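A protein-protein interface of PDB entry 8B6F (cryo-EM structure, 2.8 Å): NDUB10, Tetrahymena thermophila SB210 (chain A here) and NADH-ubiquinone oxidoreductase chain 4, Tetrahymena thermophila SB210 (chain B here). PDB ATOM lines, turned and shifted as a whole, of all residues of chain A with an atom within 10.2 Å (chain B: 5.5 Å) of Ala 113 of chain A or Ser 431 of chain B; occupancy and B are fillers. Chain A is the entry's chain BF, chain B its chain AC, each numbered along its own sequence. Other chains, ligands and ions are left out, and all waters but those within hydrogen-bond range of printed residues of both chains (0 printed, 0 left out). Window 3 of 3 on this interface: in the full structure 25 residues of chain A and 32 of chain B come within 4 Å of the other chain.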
ATOM      1  N   GLU A  64      -1.570  15.972 -11.519  1.00  0.00           N
ATOM      2  CA  GLU A  64      -2.380  15.385 -10.458  1.00  0.00           C
ATOM      3  C   GLU A  64      -3.507  14.547 -11.049  1.00  0.00           C
ATOM      4  O   GLU A  64      -3.769  13.427 -10.598  1.00  0.00           O
ATOM      5  CB  GLU A  64      -2.938  16.486  -9.557  1.00  0.00           C
ATOM      6  CG  GLU A  64      -1.875  17.308  -8.847  1.00  0.00           C
ATOM      7  CD  GLU A  64      -1.176  16.539  -7.745  1.00  0.00           C
ATOM      8  OE1 GLU A  64      -1.364  15.308  -7.659  1.00  0.00           O
ATOM      9  OE2 GLU A  64      -0.442  17.170  -6.956  1.00  0.00           O
ATOM     10  N   LEU A  65      -4.193  15.083 -12.060  1.00  0.00           N
ATOM     11  CA  LEU A  65      -5.222  14.315 -12.750  1.00  0.00           C
ATOM     12  C   LEU A  65      -4.640  13.070 -13.406  1.00  0.00           C
ATOM     13  O   LEU A  65      -5.319  12.042 -13.503  1.00  0.00           O
ATOM     14  CB  LEU A  65      -5.916  15.190 -13.794  1.00  0.00           C
ATOM     15  CG  LEU A  65      -6.720  16.372 -13.250  1.00  0.00           C
ATOM     16  CD1 LEU A  65      -7.183  17.267 -14.386  1.00  0.00           C
ATOM     17  CD2 LEU A  65      -7.909  15.891 -12.438  1.00  0.00           C
ATOM     18  N   LEU A  67      -1.974  11.254 -12.348  1.00  0.00           N
ATOM     19  CA  LEU A  67      -1.763  10.254 -11.308  1.00  0.00           C
ATOM     20  C   LEU A  67      -3.082   9.633 -10.867  1.00  0.00           C
ATOM     21  O   LEU A  67      -3.162   8.418 -10.657  1.00  0.00           O
ATOM     22  CB  LEU A  67      -1.029  10.880 -10.126  1.00  0.00           C
ATOM     23  CG  LEU A  67       0.335  11.498 -10.438  1.00  0.00           C
ATOM     24  CD1 LEU A  67       0.927  12.129  -9.194  1.00  0.00           C
ATOM     25  CD2 LEU A  67       1.288  10.465 -11.015  1.00  0.00           C
ATOM     26  N   ASN A  68      -4.126  10.448 -10.717  1.00  0.00           N
ATOM     27  CA  ASN A  68      -5.448   9.904 -10.423  1.00  0.00           C
ATOM     28  C   ASN A  68      -5.906   8.975 -11.537  1.00  0.00           C
ATOM     29  O   ASN A  68      -6.576   7.969 -11.283  1.00  0.00           O
ATOM     30  CB  ASN A  68      -6.457  11.032 -10.217  1.00  0.00           C
ATOM     31  CG  ASN A  68      -6.238  11.781  -8.921  1.00  0.00           C
ATOM     32  OD1 ASN A  68      -5.637  11.260  -7.984  1.00  0.00           O
ATOM     33  ND2 ASN A  68      -6.734  13.009  -8.857  1.00  0.00           N
ATOM     34  N   ARG A  71      -4.358   5.654 -11.037  1.00  0.00           N
ATOM     35  CA  ARG A  71      -5.075   4.898 -10.018  1.00  0.00           C
ATOM     36  C   ARG A  71      -6.371   4.323 -10.577  1.00  0.00           C
ATOM     37  O   ARG A  71      -6.726   3.174 -10.291  1.00  0.00           O
ATOM     38  CB  ARG A  71      -5.357   5.786  -8.807  1.00  0.00           C
ATOM     39  CG  ARG A  71      -5.828   5.026  -7.577  1.00  0.00           C
ATOM     40  CD  ARG A  71      -4.754   4.064  -7.096  1.00  0.00           C
ATOM     41  NE  ARG A  71      -5.045   3.510  -5.779  1.00  0.00           N
ATOM     42  CZ  ARG A  71      -5.698   2.378  -5.563  1.00  0.00           C
ATOM     43  NH1 ARG A  71      -6.166   1.647  -6.561  1.00  0.00           N
ATOM     44  NH2 ARG A  71      -5.886   1.967  -4.313  1.00  0.00           N
ATOM     45  N   LYS A  72      -7.112   5.122 -11.344  1.00  0.00           N
ATOM     46  CA  LYS A  72      -8.352   4.634 -11.936  1.00  0.00           C
ATOM     47  C   LYS A  72      -8.085   3.487 -12.901  1.00  0.00           C
ATOM     48  O   LYS A  72      -8.836   2.507 -12.936  1.00  0.00           O
ATOM     49  CB  LYS A  72      -9.074   5.776 -12.648  1.00  0.00           C
ATOM     50  CG  LYS A  72      -9.535   6.882 -11.716  1.00  0.00           C
ATOM     51  CD  LYS A  72      -9.736   8.192 -12.458  1.00  0.00           C
ATOM     52  CE  LYS A  72     -10.782   8.063 -13.551  1.00  0.00           C
ATOM     53  NZ  LYS A  72     -10.993   9.352 -14.261  1.00  0.00           N
ATOM     54  N   LEU A 105       0.395   3.424  -5.661  1.00  0.00           N
ATOM     55  CA  LEU A 105      -0.485   4.520  -6.048  1.00  0.00           C
ATOM     56  C   LEU A 105      -1.456   4.893  -4.934  1.00  0.00           C
ATOM     57  O   LEU A 105      -2.598   5.272  -5.207  1.00  0.00           O
ATOM     58  CB  LEU A 105      -1.250   4.158  -7.320  1.00  0.00           C
ATOM     59  CG  LEU A 105      -0.407   3.883  -8.565  1.00  0.00           C
ATOM     60  CD1 LEU A 105      -1.283   3.379  -9.695  1.00  0.00           C
ATOM     61  CD2 LEU A 105       0.347   5.129  -8.997  1.00  0.00           C
ATOM     62  N   SER A 106      -1.026   4.787  -3.680  1.00  0.00           N
ATOM     63  CA  SER A 106      -1.892   5.077  -2.549  1.00  0.00           C
ATOM     64  C   SER A 106      -2.075   6.584  -2.390  1.00  0.00           C
ATOM     65  O   SER A 106      -1.571   7.389  -3.177  1.00  0.00           O
ATOM     66  CB  SER A 106      -1.324   4.457  -1.276  1.00  0.00           C
ATOM     67  OG  SER A 106      -1.238   3.047  -1.394  1.00  0.00           O
ATOM     68  N   SER A 107      -2.806   6.970  -1.344  1.00  0.00           N
ATOM     69  CA  SER A 107      -3.185   8.370  -1.183  1.00  0.00           C
ATOM     70  C   SER A 107      -1.996   9.319  -1.140  1.00  0.00           C
ATOM     71  O   SER A 107      -2.079  10.390  -1.769  1.00  0.00           O
ATOM     72  CB  SER A 107      -4.048   8.534   0.075  1.00  0.00           C
ATOM     73  OG  SER A 107      -3.277   8.408   1.256  1.00  0.00           O
ATOM     74  N   PRO A 108      -0.895   9.028  -0.441  1.00  0.00           N
ATOM     75  CA  PRO A 108       0.207  10.004  -0.407  1.00  0.00           C
ATOM     76  C   PRO A 108       0.760  10.317  -1.783  1.00  0.00           C
ATOM     77  O   PRO A 108       1.214  11.442  -2.023  1.00  0.00           O
ATOM     78  CB  PRO A 108       1.260   9.323   0.482  1.00  0.00           C
ATOM     79  CG  PRO A 108       0.536   8.229   1.191  1.00  0.00           C
ATOM     80  CD  PRO A 108      -0.532   7.782   0.253  1.00  0.00           C
ATOM     81  N   HIS A 109       0.729   9.350  -2.697  1.00  0.00           N
ATOM     82  CA  HIS A 109       1.312   9.518  -4.020  1.00  0.00           C
ATOM     83  C   HIS A 109       0.308  10.021  -5.044  1.00  0.00           C
ATOM     84  O   HIS A 109       0.703  10.667  -6.020  1.00  0.00           O
ATOM     85  CB  HIS A 109       1.905   8.189  -4.494  1.00  0.00           C
ATOM     86  CG  HIS A 109       2.628   7.442  -3.417  1.00  0.00           C
ATOM     87  ND1 HIS A 109       3.924   7.734  -3.049  1.00  0.00           N
ATOM     88  CD2 HIS A 109       2.235   6.419  -2.625  1.00  0.00           C
ATOM     89  CE1 HIS A 109       4.297   6.921  -2.078  1.00  0.00           C
ATOM     90  NE2 HIS A 109       3.290   6.113  -1.801  1.00  0.00           N
ATOM     91  N   VAL A 110      -0.978   9.739  -4.850  1.00  0.00           N
ATOM     92  CA  VAL A 110      -2.031  10.227  -5.730  1.00  0.00           C
ATOM     93  C   VAL A 110      -3.139  10.809  -4.865  1.00  0.00           C
ATOM     94  O   VAL A 110      -3.569  10.181  -3.892  1.00  0.00           O
ATOM     95  CB  VAL A 110      -2.575   9.109  -6.644  1.00  0.00           C
ATOM     96  CG1 VAL A 110      -1.427   8.374  -7.315  1.00  0.00           C
ATOM     97  CG2 VAL A 110      -3.457   8.131  -5.876  1.00  0.00           C
ATOM     98  N   ARG A 111      -3.587  12.014  -5.208  1.00  0.00           N
ATOM     99  CA  ARG A 111      -4.650  12.693  -4.469  1.00  0.00           C
ATOM    100  C   ARG A 111      -5.981  12.232  -5.046  1.00  0.00           C
ATOM    101  O   ARG A 111      -6.504  12.809  -6.000  1.00  0.00           O
ATOM    102  CB  ARG A 111      -4.479  14.202  -4.560  1.00  0.00           C
ATOM    103  CG  ARG A 111      -5.589  15.019  -3.912  1.00  0.00           C
ATOM    104  CD  ARG A 111      -5.819  16.314  -4.670  1.00  0.00           C
ATOM    105  NE  ARG A 111      -6.298  16.068  -6.024  1.00  0.00           N
ATOM    106  CZ  ARG A 111      -6.340  16.980  -6.984  1.00  0.00           C
ATOM    107  NH1 ARG A 111      -5.926  18.219  -6.781  1.00  0.00           N
ATOM    108  NH2 ARG A 111      -6.813  16.641  -8.180  1.00  0.00           N
ATOM    109  N   GLY A 112      -6.538  11.178  -4.462  1.00  0.00           N
ATOM    110  CA  GLY A 112      -7.792  10.646  -4.953  1.00  0.00           C
ATOM    111  C   GLY A 112      -8.926  11.644  -4.861  1.00  0.00           C
ATOM    112  O   GLY A 112      -9.396  12.154  -5.881  1.00  0.00           O
ATOM    113  N   ALA A 113      -9.354  11.953  -3.638  1.00  0.00           N
ATOM    114  CA  ALA A 113     -10.477  12.849  -3.417  1.00  0.00           C
ATOM    115  C   ALA A 113     -10.178  13.925  -2.387  1.00  0.00           C
ATOM    116  O   ALA A 113     -11.079  14.696  -2.043  1.00  0.00           O
ATOM    117  CB  ALA A 113     -11.715  12.056  -2.975  1.00  0.00           C
ATOM    118  N   HIS A 114      -8.949  14.000  -1.891  1.00  0.00           N
ATOM    119  CA  HIS A 114      -8.593  15.001  -0.901  1.00  0.00           C
ATOM    120  C   HIS A 114      -8.655  16.393  -1.516  1.00  0.00           C
ATOM    121  O   HIS A 114      -8.416  16.580  -2.710  1.00  0.00           O
ATOM    122  CB  HIS A 114      -7.196  14.728  -0.351  1.00  0.00           C
ATOM    123  CG  HIS A 114      -6.992  13.313   0.091  1.00  0.00           C
ATOM    124  ND1 HIS A 114      -8.040  12.457   0.356  1.00  0.00           N
ATOM    125  CD2 HIS A 114      -5.863  12.599   0.302  1.00  0.00           C
ATOM    126  CE1 HIS A 114      -7.565  11.280   0.715  1.00  0.00           C
ATOM    127  NE2 HIS A 114      -6.246  11.338   0.692  1.00  0.00           N
ATOM    128  N   PHE A 115      -8.988  17.377  -0.681  1.00  0.00           N
ATOM    129  CA  PHE A 115      -9.092  18.747  -1.168  1.00  0.00           C
ATOM    130  C   PHE A 115      -7.775  19.218  -1.767  1.00  0.00           C
ATOM    131  O   PHE A 115      -7.759  19.850  -2.830  1.00  0.00           O
ATOM    132  CB  PHE A 115      -9.520  19.679  -0.032  1.00  0.00           C
ATOM    133  CG  PHE A 115     -10.985  19.609   0.311  1.00  0.00           C
ATOM    134  CD1 PHE A 115     -11.945  19.408  -0.669  1.00  0.00           C
ATOM    135  CD2 PHE A 115     -11.401  19.771   1.621  1.00  0.00           C
ATOM    136  CE1 PHE A 115     -13.287  19.356  -0.346  1.00  0.00           C
ATOM    137  CE2 PHE A 115     -12.740  19.721   1.950  1.00  0.00           C
ATOM    138  CZ  PHE A 115     -13.685  19.515   0.966  1.00  0.00           C
ATOM    139  N   GLN A 116      -6.661  18.922  -1.104  1.00  0.00           N
ATOM    140  CA  GLN A 116      -5.351  19.388  -1.529  1.00  0.00           C
ATOM    141  C   GLN A 116      -4.348  18.249  -1.461  1.00  0.00           C
ATOM    142  O   GLN A 116      -4.324  17.487  -0.491  1.00  0.00           O
ATOM    143  CB  GLN A 116      -4.867  20.551  -0.654  1.00  0.00           C
ATOM    144  CG  GLN A 116      -3.522  21.128  -1.065  1.00  0.00           C
ATOM    145  CD  GLN A 116      -3.600  21.928  -2.347  1.00  0.00           C
ATOM    146  OE1 GLN A 116      -3.641  23.157  -2.319  1.00  0.00           O
ATOM    147  NE2 GLN A 116      -3.615  21.238  -3.480  1.00  0.00           N
ATOM    148  N   ALA A 117      -3.523  18.140  -2.498  1.00  0.00           N
ATOM    149  CA  ALA A 117      -2.364  17.256  -2.488  1.00  0.00           C
ATOM    150  C   ALA A 117      -1.198  18.029  -1.891  1.00  0.00           C
ATOM    151  O   ALA A 117      -0.641  18.921  -2.538  1.00  0.00           O
ATOM    152  CB  ALA A 117      -2.036  16.777  -3.900  1.00  0.00           C
ATOM    153  N   ARG A 119       2.052  18.966  -1.437  1.00  0.00           N
ATOM    154  CA  ARG A 119       3.291  18.755  -2.169  1.00  0.00           C
ATOM    155  C   ARG A 119       4.227  19.919  -1.896  1.00  0.00           C
ATOM    156  O   ARG A 119       3.811  21.081  -1.954  1.00  0.00           O
ATOM    157  CB  ARG A 119       3.026  18.641  -3.674  1.00  0.00           C
ATOM    158  CG  ARG A 119       2.068  17.526  -4.072  1.00  0.00           C
ATOM    159  CD  ARG A 119       2.800  16.217  -4.316  1.00  0.00           C
ATOM    160  NE  ARG A 119       1.937  15.224  -4.947  1.00  0.00           N
ATOM    161  CZ  ARG A 119       1.269  14.274  -4.304  1.00  0.00           C
ATOM    162  NH1 ARG A 119       1.340  14.144  -2.990  1.00  0.00           N
ATOM    163  NH2 ARG A 119       0.510  13.434  -4.999  1.00  0.00           N
ATOM    164  N   GLU B 426     -22.553  16.893  -1.846  1.00  0.00           N
ATOM    165  CA  GLU B 426     -22.292  16.278  -0.550  1.00  0.00           C
ATOM    166  C   GLU B 426     -21.108  15.326  -0.636  1.00  0.00           C
ATOM    167  O   GLU B 426     -20.263  15.289   0.264  1.00  0.00           O
ATOM    168  CB  GLU B 426     -23.538  15.546  -0.057  1.00  0.00           C
ATOM    169  CG  GLU B 426     -24.643  16.477   0.417  1.00  0.00           C
ATOM    170  CD  GLU B 426     -25.846  15.727   0.957  1.00  0.00           C
ATOM    171  OE1 GLU B 426     -25.897  14.489   0.802  1.00  0.00           O
ATOM    172  OE2 GLU B 426     -26.742  16.375   1.538  1.00  0.00           O
ATOM    173  N   PHE B 427     -21.030  14.550  -1.718  1.00  0.00           N
ATOM    174  CA  PHE B 427     -19.924  13.614  -1.882  1.00  0.00           C
ATOM    175  C   PHE B 427     -18.593  14.355  -1.957  1.00  0.00           C
ATOM    176  O   PHE B 427     -17.621  13.971  -1.297  1.00  0.00           O
ATOM    177  CB  PHE B 427     -20.148  12.769  -3.136  1.00  0.00           C
ATOM    178  CG  PHE B 427     -19.341  11.505  -3.166  1.00  0.00           C
ATOM    179  CD1 PHE B 427     -19.813  10.357  -2.552  1.00  0.00           C
ATOM    180  CD2 PHE B 427     -18.121  11.458  -3.817  1.00  0.00           C
ATOM    181  CE1 PHE B 427     -19.082   9.188  -2.579  1.00  0.00           C
ATOM    182  CE2 PHE B 427     -17.384  10.289  -3.849  1.00  0.00           C
ATOM    183  CZ  PHE B 427     -17.866   9.154  -3.228  1.00  0.00           C
ATOM    184  N   TYR B 428     -18.526  15.415  -2.766  1.00  0.00           N
ATOM    185  CA  TYR B 428     -17.298  16.203  -2.851  1.00  0.00           C
ATOM    186  C   TYR B 428     -16.879  16.714  -1.478  1.00  0.00           C
ATOM    187  O   TYR B 428     -15.741  16.510  -1.044  1.00  0.00           O
ATOM    188  CB  TYR B 428     -17.499  17.390  -3.794  1.00  0.00           C
ATOM    189  CG  TYR B 428     -17.173  17.142  -5.248  1.00  0.00           C
ATOM    190  CD1 TYR B 428     -18.065  16.482  -6.080  1.00  0.00           C
ATOM    191  CD2 TYR B 428     -15.990  17.618  -5.798  1.00  0.00           C
ATOM    192  CE1 TYR B 428     -17.776  16.276  -7.413  1.00  0.00           C
ATOM    193  CE2 TYR B 428     -15.693  17.418  -7.130  1.00  0.00           C
ATOM    194  CZ  TYR B 428     -16.590  16.746  -7.933  1.00  0.00           C
ATOM    195  OH  TYR B 428     -16.300  16.544  -9.260  1.00  0.00           O
ATOM    196  N   ILE B 429     -17.792  17.398  -0.785  1.00  0.00           N
ATOM    197  CA  ILE B 429     -17.433  18.068   0.461  1.00  0.00           C
ATOM    198  C   ILE B 429     -17.034  17.052   1.518  1.00  0.00           C
ATOM    199  O   ILE B 429     -16.040  17.229   2.230  1.00  0.00           O
ATOM    200  CB  ILE B 429     -18.597  18.957   0.940  1.00  0.00           C
ATOM    201  CG1 ILE B 429     -18.917  20.036  -0.100  1.00  0.00           C
ATOM    202  CG2 ILE B 429     -18.274  19.592   2.289  1.00  0.00           C
ATOM    203  CD1 ILE B 429     -17.763  20.959  -0.425  1.00  0.00           C
ATOM    204  N   PHE B 430     -17.806  15.971   1.643  1.00  0.00           N
ATOM    205  CA  PHE B 430     -17.520  14.977   2.667  1.00  0.00           C
ATOM    206  C   PHE B 430     -16.269  14.175   2.344  1.00  0.00           C
ATOM    207  O   PHE B 430     -15.531  13.794   3.259  1.00  0.00           O
ATOM    208  CB  PHE B 430     -18.722  14.048   2.846  1.00  0.00           C
ATOM    209  CG  PHE B 430     -19.994  14.760   3.218  1.00  0.00           C
ATOM    210  CD1 PHE B 430     -19.964  16.001   3.836  1.00  0.00           C
ATOM    211  CD2 PHE B 430     -21.224  14.181   2.955  1.00  0.00           C
ATOM    212  CE1 PHE B 430     -21.134  16.650   4.179  1.00  0.00           C
ATOM    213  CE2 PHE B 430     -22.398  14.826   3.296  1.00  0.00           C
ATOM    214  CZ  PHE B 430     -22.352  16.060   3.909  1.00  0.00           C
ATOM    215  N   SER B 431     -16.007  13.905   1.064  1.00  0.00           N
ATOM    216  CA  SER B 431     -14.770  13.216   0.713  1.00  0.00           C
ATOM    217  C   SER B 431     -13.553  14.041   1.100  1.00  0.00           C
ATOM    218  O   SER B 431     -12.564  13.502   1.609  1.00  0.00           O
ATOM    219  CB  SER B 431     -14.748  12.915  -0.785  1.00  0.00           C
ATOM    220  OG  SER B 431     -15.837  12.090  -1.158  1.00  0.00           O
ATOM    221  N   GLY B 432     -13.596  15.349   0.854  1.00  0.00           N
ATOM    222  CA  GLY B 432     -12.511  16.207   1.296  1.00  0.00           C
ATOM    223  C   GLY B 432     -12.416  16.305   2.806  1.00  0.00           C
ATOM    224  O   GLY B 432     -11.324  16.228   3.375  1.00  0.00           O
ATOM    225  N   LEU B 433     -13.559  16.479   3.478  1.00  0.00           N
ATOM    226  CA  LEU B 433     -13.548  16.678   4.923  1.00  0.00           C
ATOM    227  C   LEU B 433     -13.128  15.420   5.666  1.00  0.00           C
ATOM    228  O   LEU B 433     -12.603  15.510   6.780  1.00  0.00           O
ATOM    229  CB  LEU B 433     -14.925  17.127   5.410  1.00  0.00           C
ATOM    230  CG  LEU B 433     -15.323  18.581   5.153  1.00  0.00           C
ATOM    231  CD1 LEU B 433     -16.764  18.816   5.571  1.00  0.00           C
ATOM    232  CD2 LEU B 433     -14.404  19.533   5.893  1.00  0.00           C
ATOM    233  N   LEU B 434     -13.355  14.246   5.079  1.00  0.00           N
ATOM    234  CA  LEU B 434     -12.945  13.014   5.741  1.00  0.00           C
ATOM    235  C   LEU B 434     -11.435  12.974   5.919  1.00  0.00           C
ATOM    236  O   LEU B 434     -10.937  12.583   6.981  1.00  0.00           O
ATOM    237  CB  LEU B 434     -13.437  11.802   4.951  1.00  0.00           C
ATOM    238  CG  LEU B 434     -13.179  10.439   5.595  1.00  0.00           C
ATOM    239  CD1 LEU B 434     -13.888  10.313   6.929  1.00  0.00           C
ATOM    240  CD2 LEU B 434     -13.639   9.335   4.681  1.00  0.00           C
ATOM    241  N   GLU B 435     -10.687  13.373   4.890  1.00  0.00           N
ATOM    242  CA  GLU B 435      -9.237  13.441   5.014  1.00  0.00           C
ATOM    243  C   GLU B 435      -8.785  14.677   5.784  1.00  0.00           C
ATOM    244  O   GLU B 435      -7.767  14.624   6.484  1.00  0.00           O
ATOM    245  CB  GLU B 435      -8.597  13.418   3.626  1.00  0.00           C
ATOM    246  CG  GLU B 435      -7.078  13.440   3.645  1.00  0.00           C
ATOM    247  CD  GLU B 435      -6.511  14.844   3.576  1.00  0.00           C
ATOM    248  OE1 GLU B 435      -7.085  15.686   2.853  1.00  0.00           O
ATOM    249  OE2 GLU B 435      -5.490  15.108   4.244  1.00  0.00           O
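The backbone carbonyl oxygen (O) of Phe 427 of chain B lies within hydrogen-bond range of the side-chain hydroxyl (OG) of Ser 431 of chain B (2.6 Å).
Among the printed residues, merely in contact across the chains: Ala 113 of chain A with Ser 431 of chain B, Ala 113 of chain A with Gly 432 of chain B, His 114 of chain A with Glu 435 of chain B, Phe 115 of chain A with Tyr 428 of chain B, Phe 115 of chain A with Ile 429 of chain B, Phe 115 of chain A with Gly 432 of chain B and Phe 115 of chain A with Leu 433 of chain B.
Ala 113 of chain A touches just these residues of chain B: Ser 431 and Gly 432. Of the printed residues of chain A, Ser 431 of chain B touches Ala 113. Of chain A, only Ala 113 (3.9 Å) and Phe 115 (3.5 Å) come within 4 Å of Gly 432 of chain B. Printed residues of chain A within 4 Å of Tyr 428 of chain B: Phe 115. Of the printed residues of chain B, Phe 115 of chain A touches Tyr 428 (3.8 Å), Ile 429 (3.5 Å), Gly 432 (3.5 Å) and Leu 433 (3.7 Å). Printed residues of chain A within 4 Å of Glu 435 of chain B: His 114. Of the printed residues of chain B, His 114 of chain A touches Glu 435 (3.3 Å). Printed residues of chain A within 4 Å of Leu 433 of chain B: Phe 115. Ser 107 of chain A touches none of the printed residues of chain B.
Printed residues of chain A that touch a printed residue of chain B: Ala 113, His 114 and Phe 115. Of the 10 printed residues of chain B, 6 touch a printed residue of chain A. Printed residues of chain B that touch a printed residue of chain A: Tyr 428, Ile 429, Ser 431, Gly 432, Leu 433 and Glu 435. Among the printed residues, no Asp or Glu carboxylate lies within 4 Å of a Lys or Arg side-chain nitrogen of the other chain.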
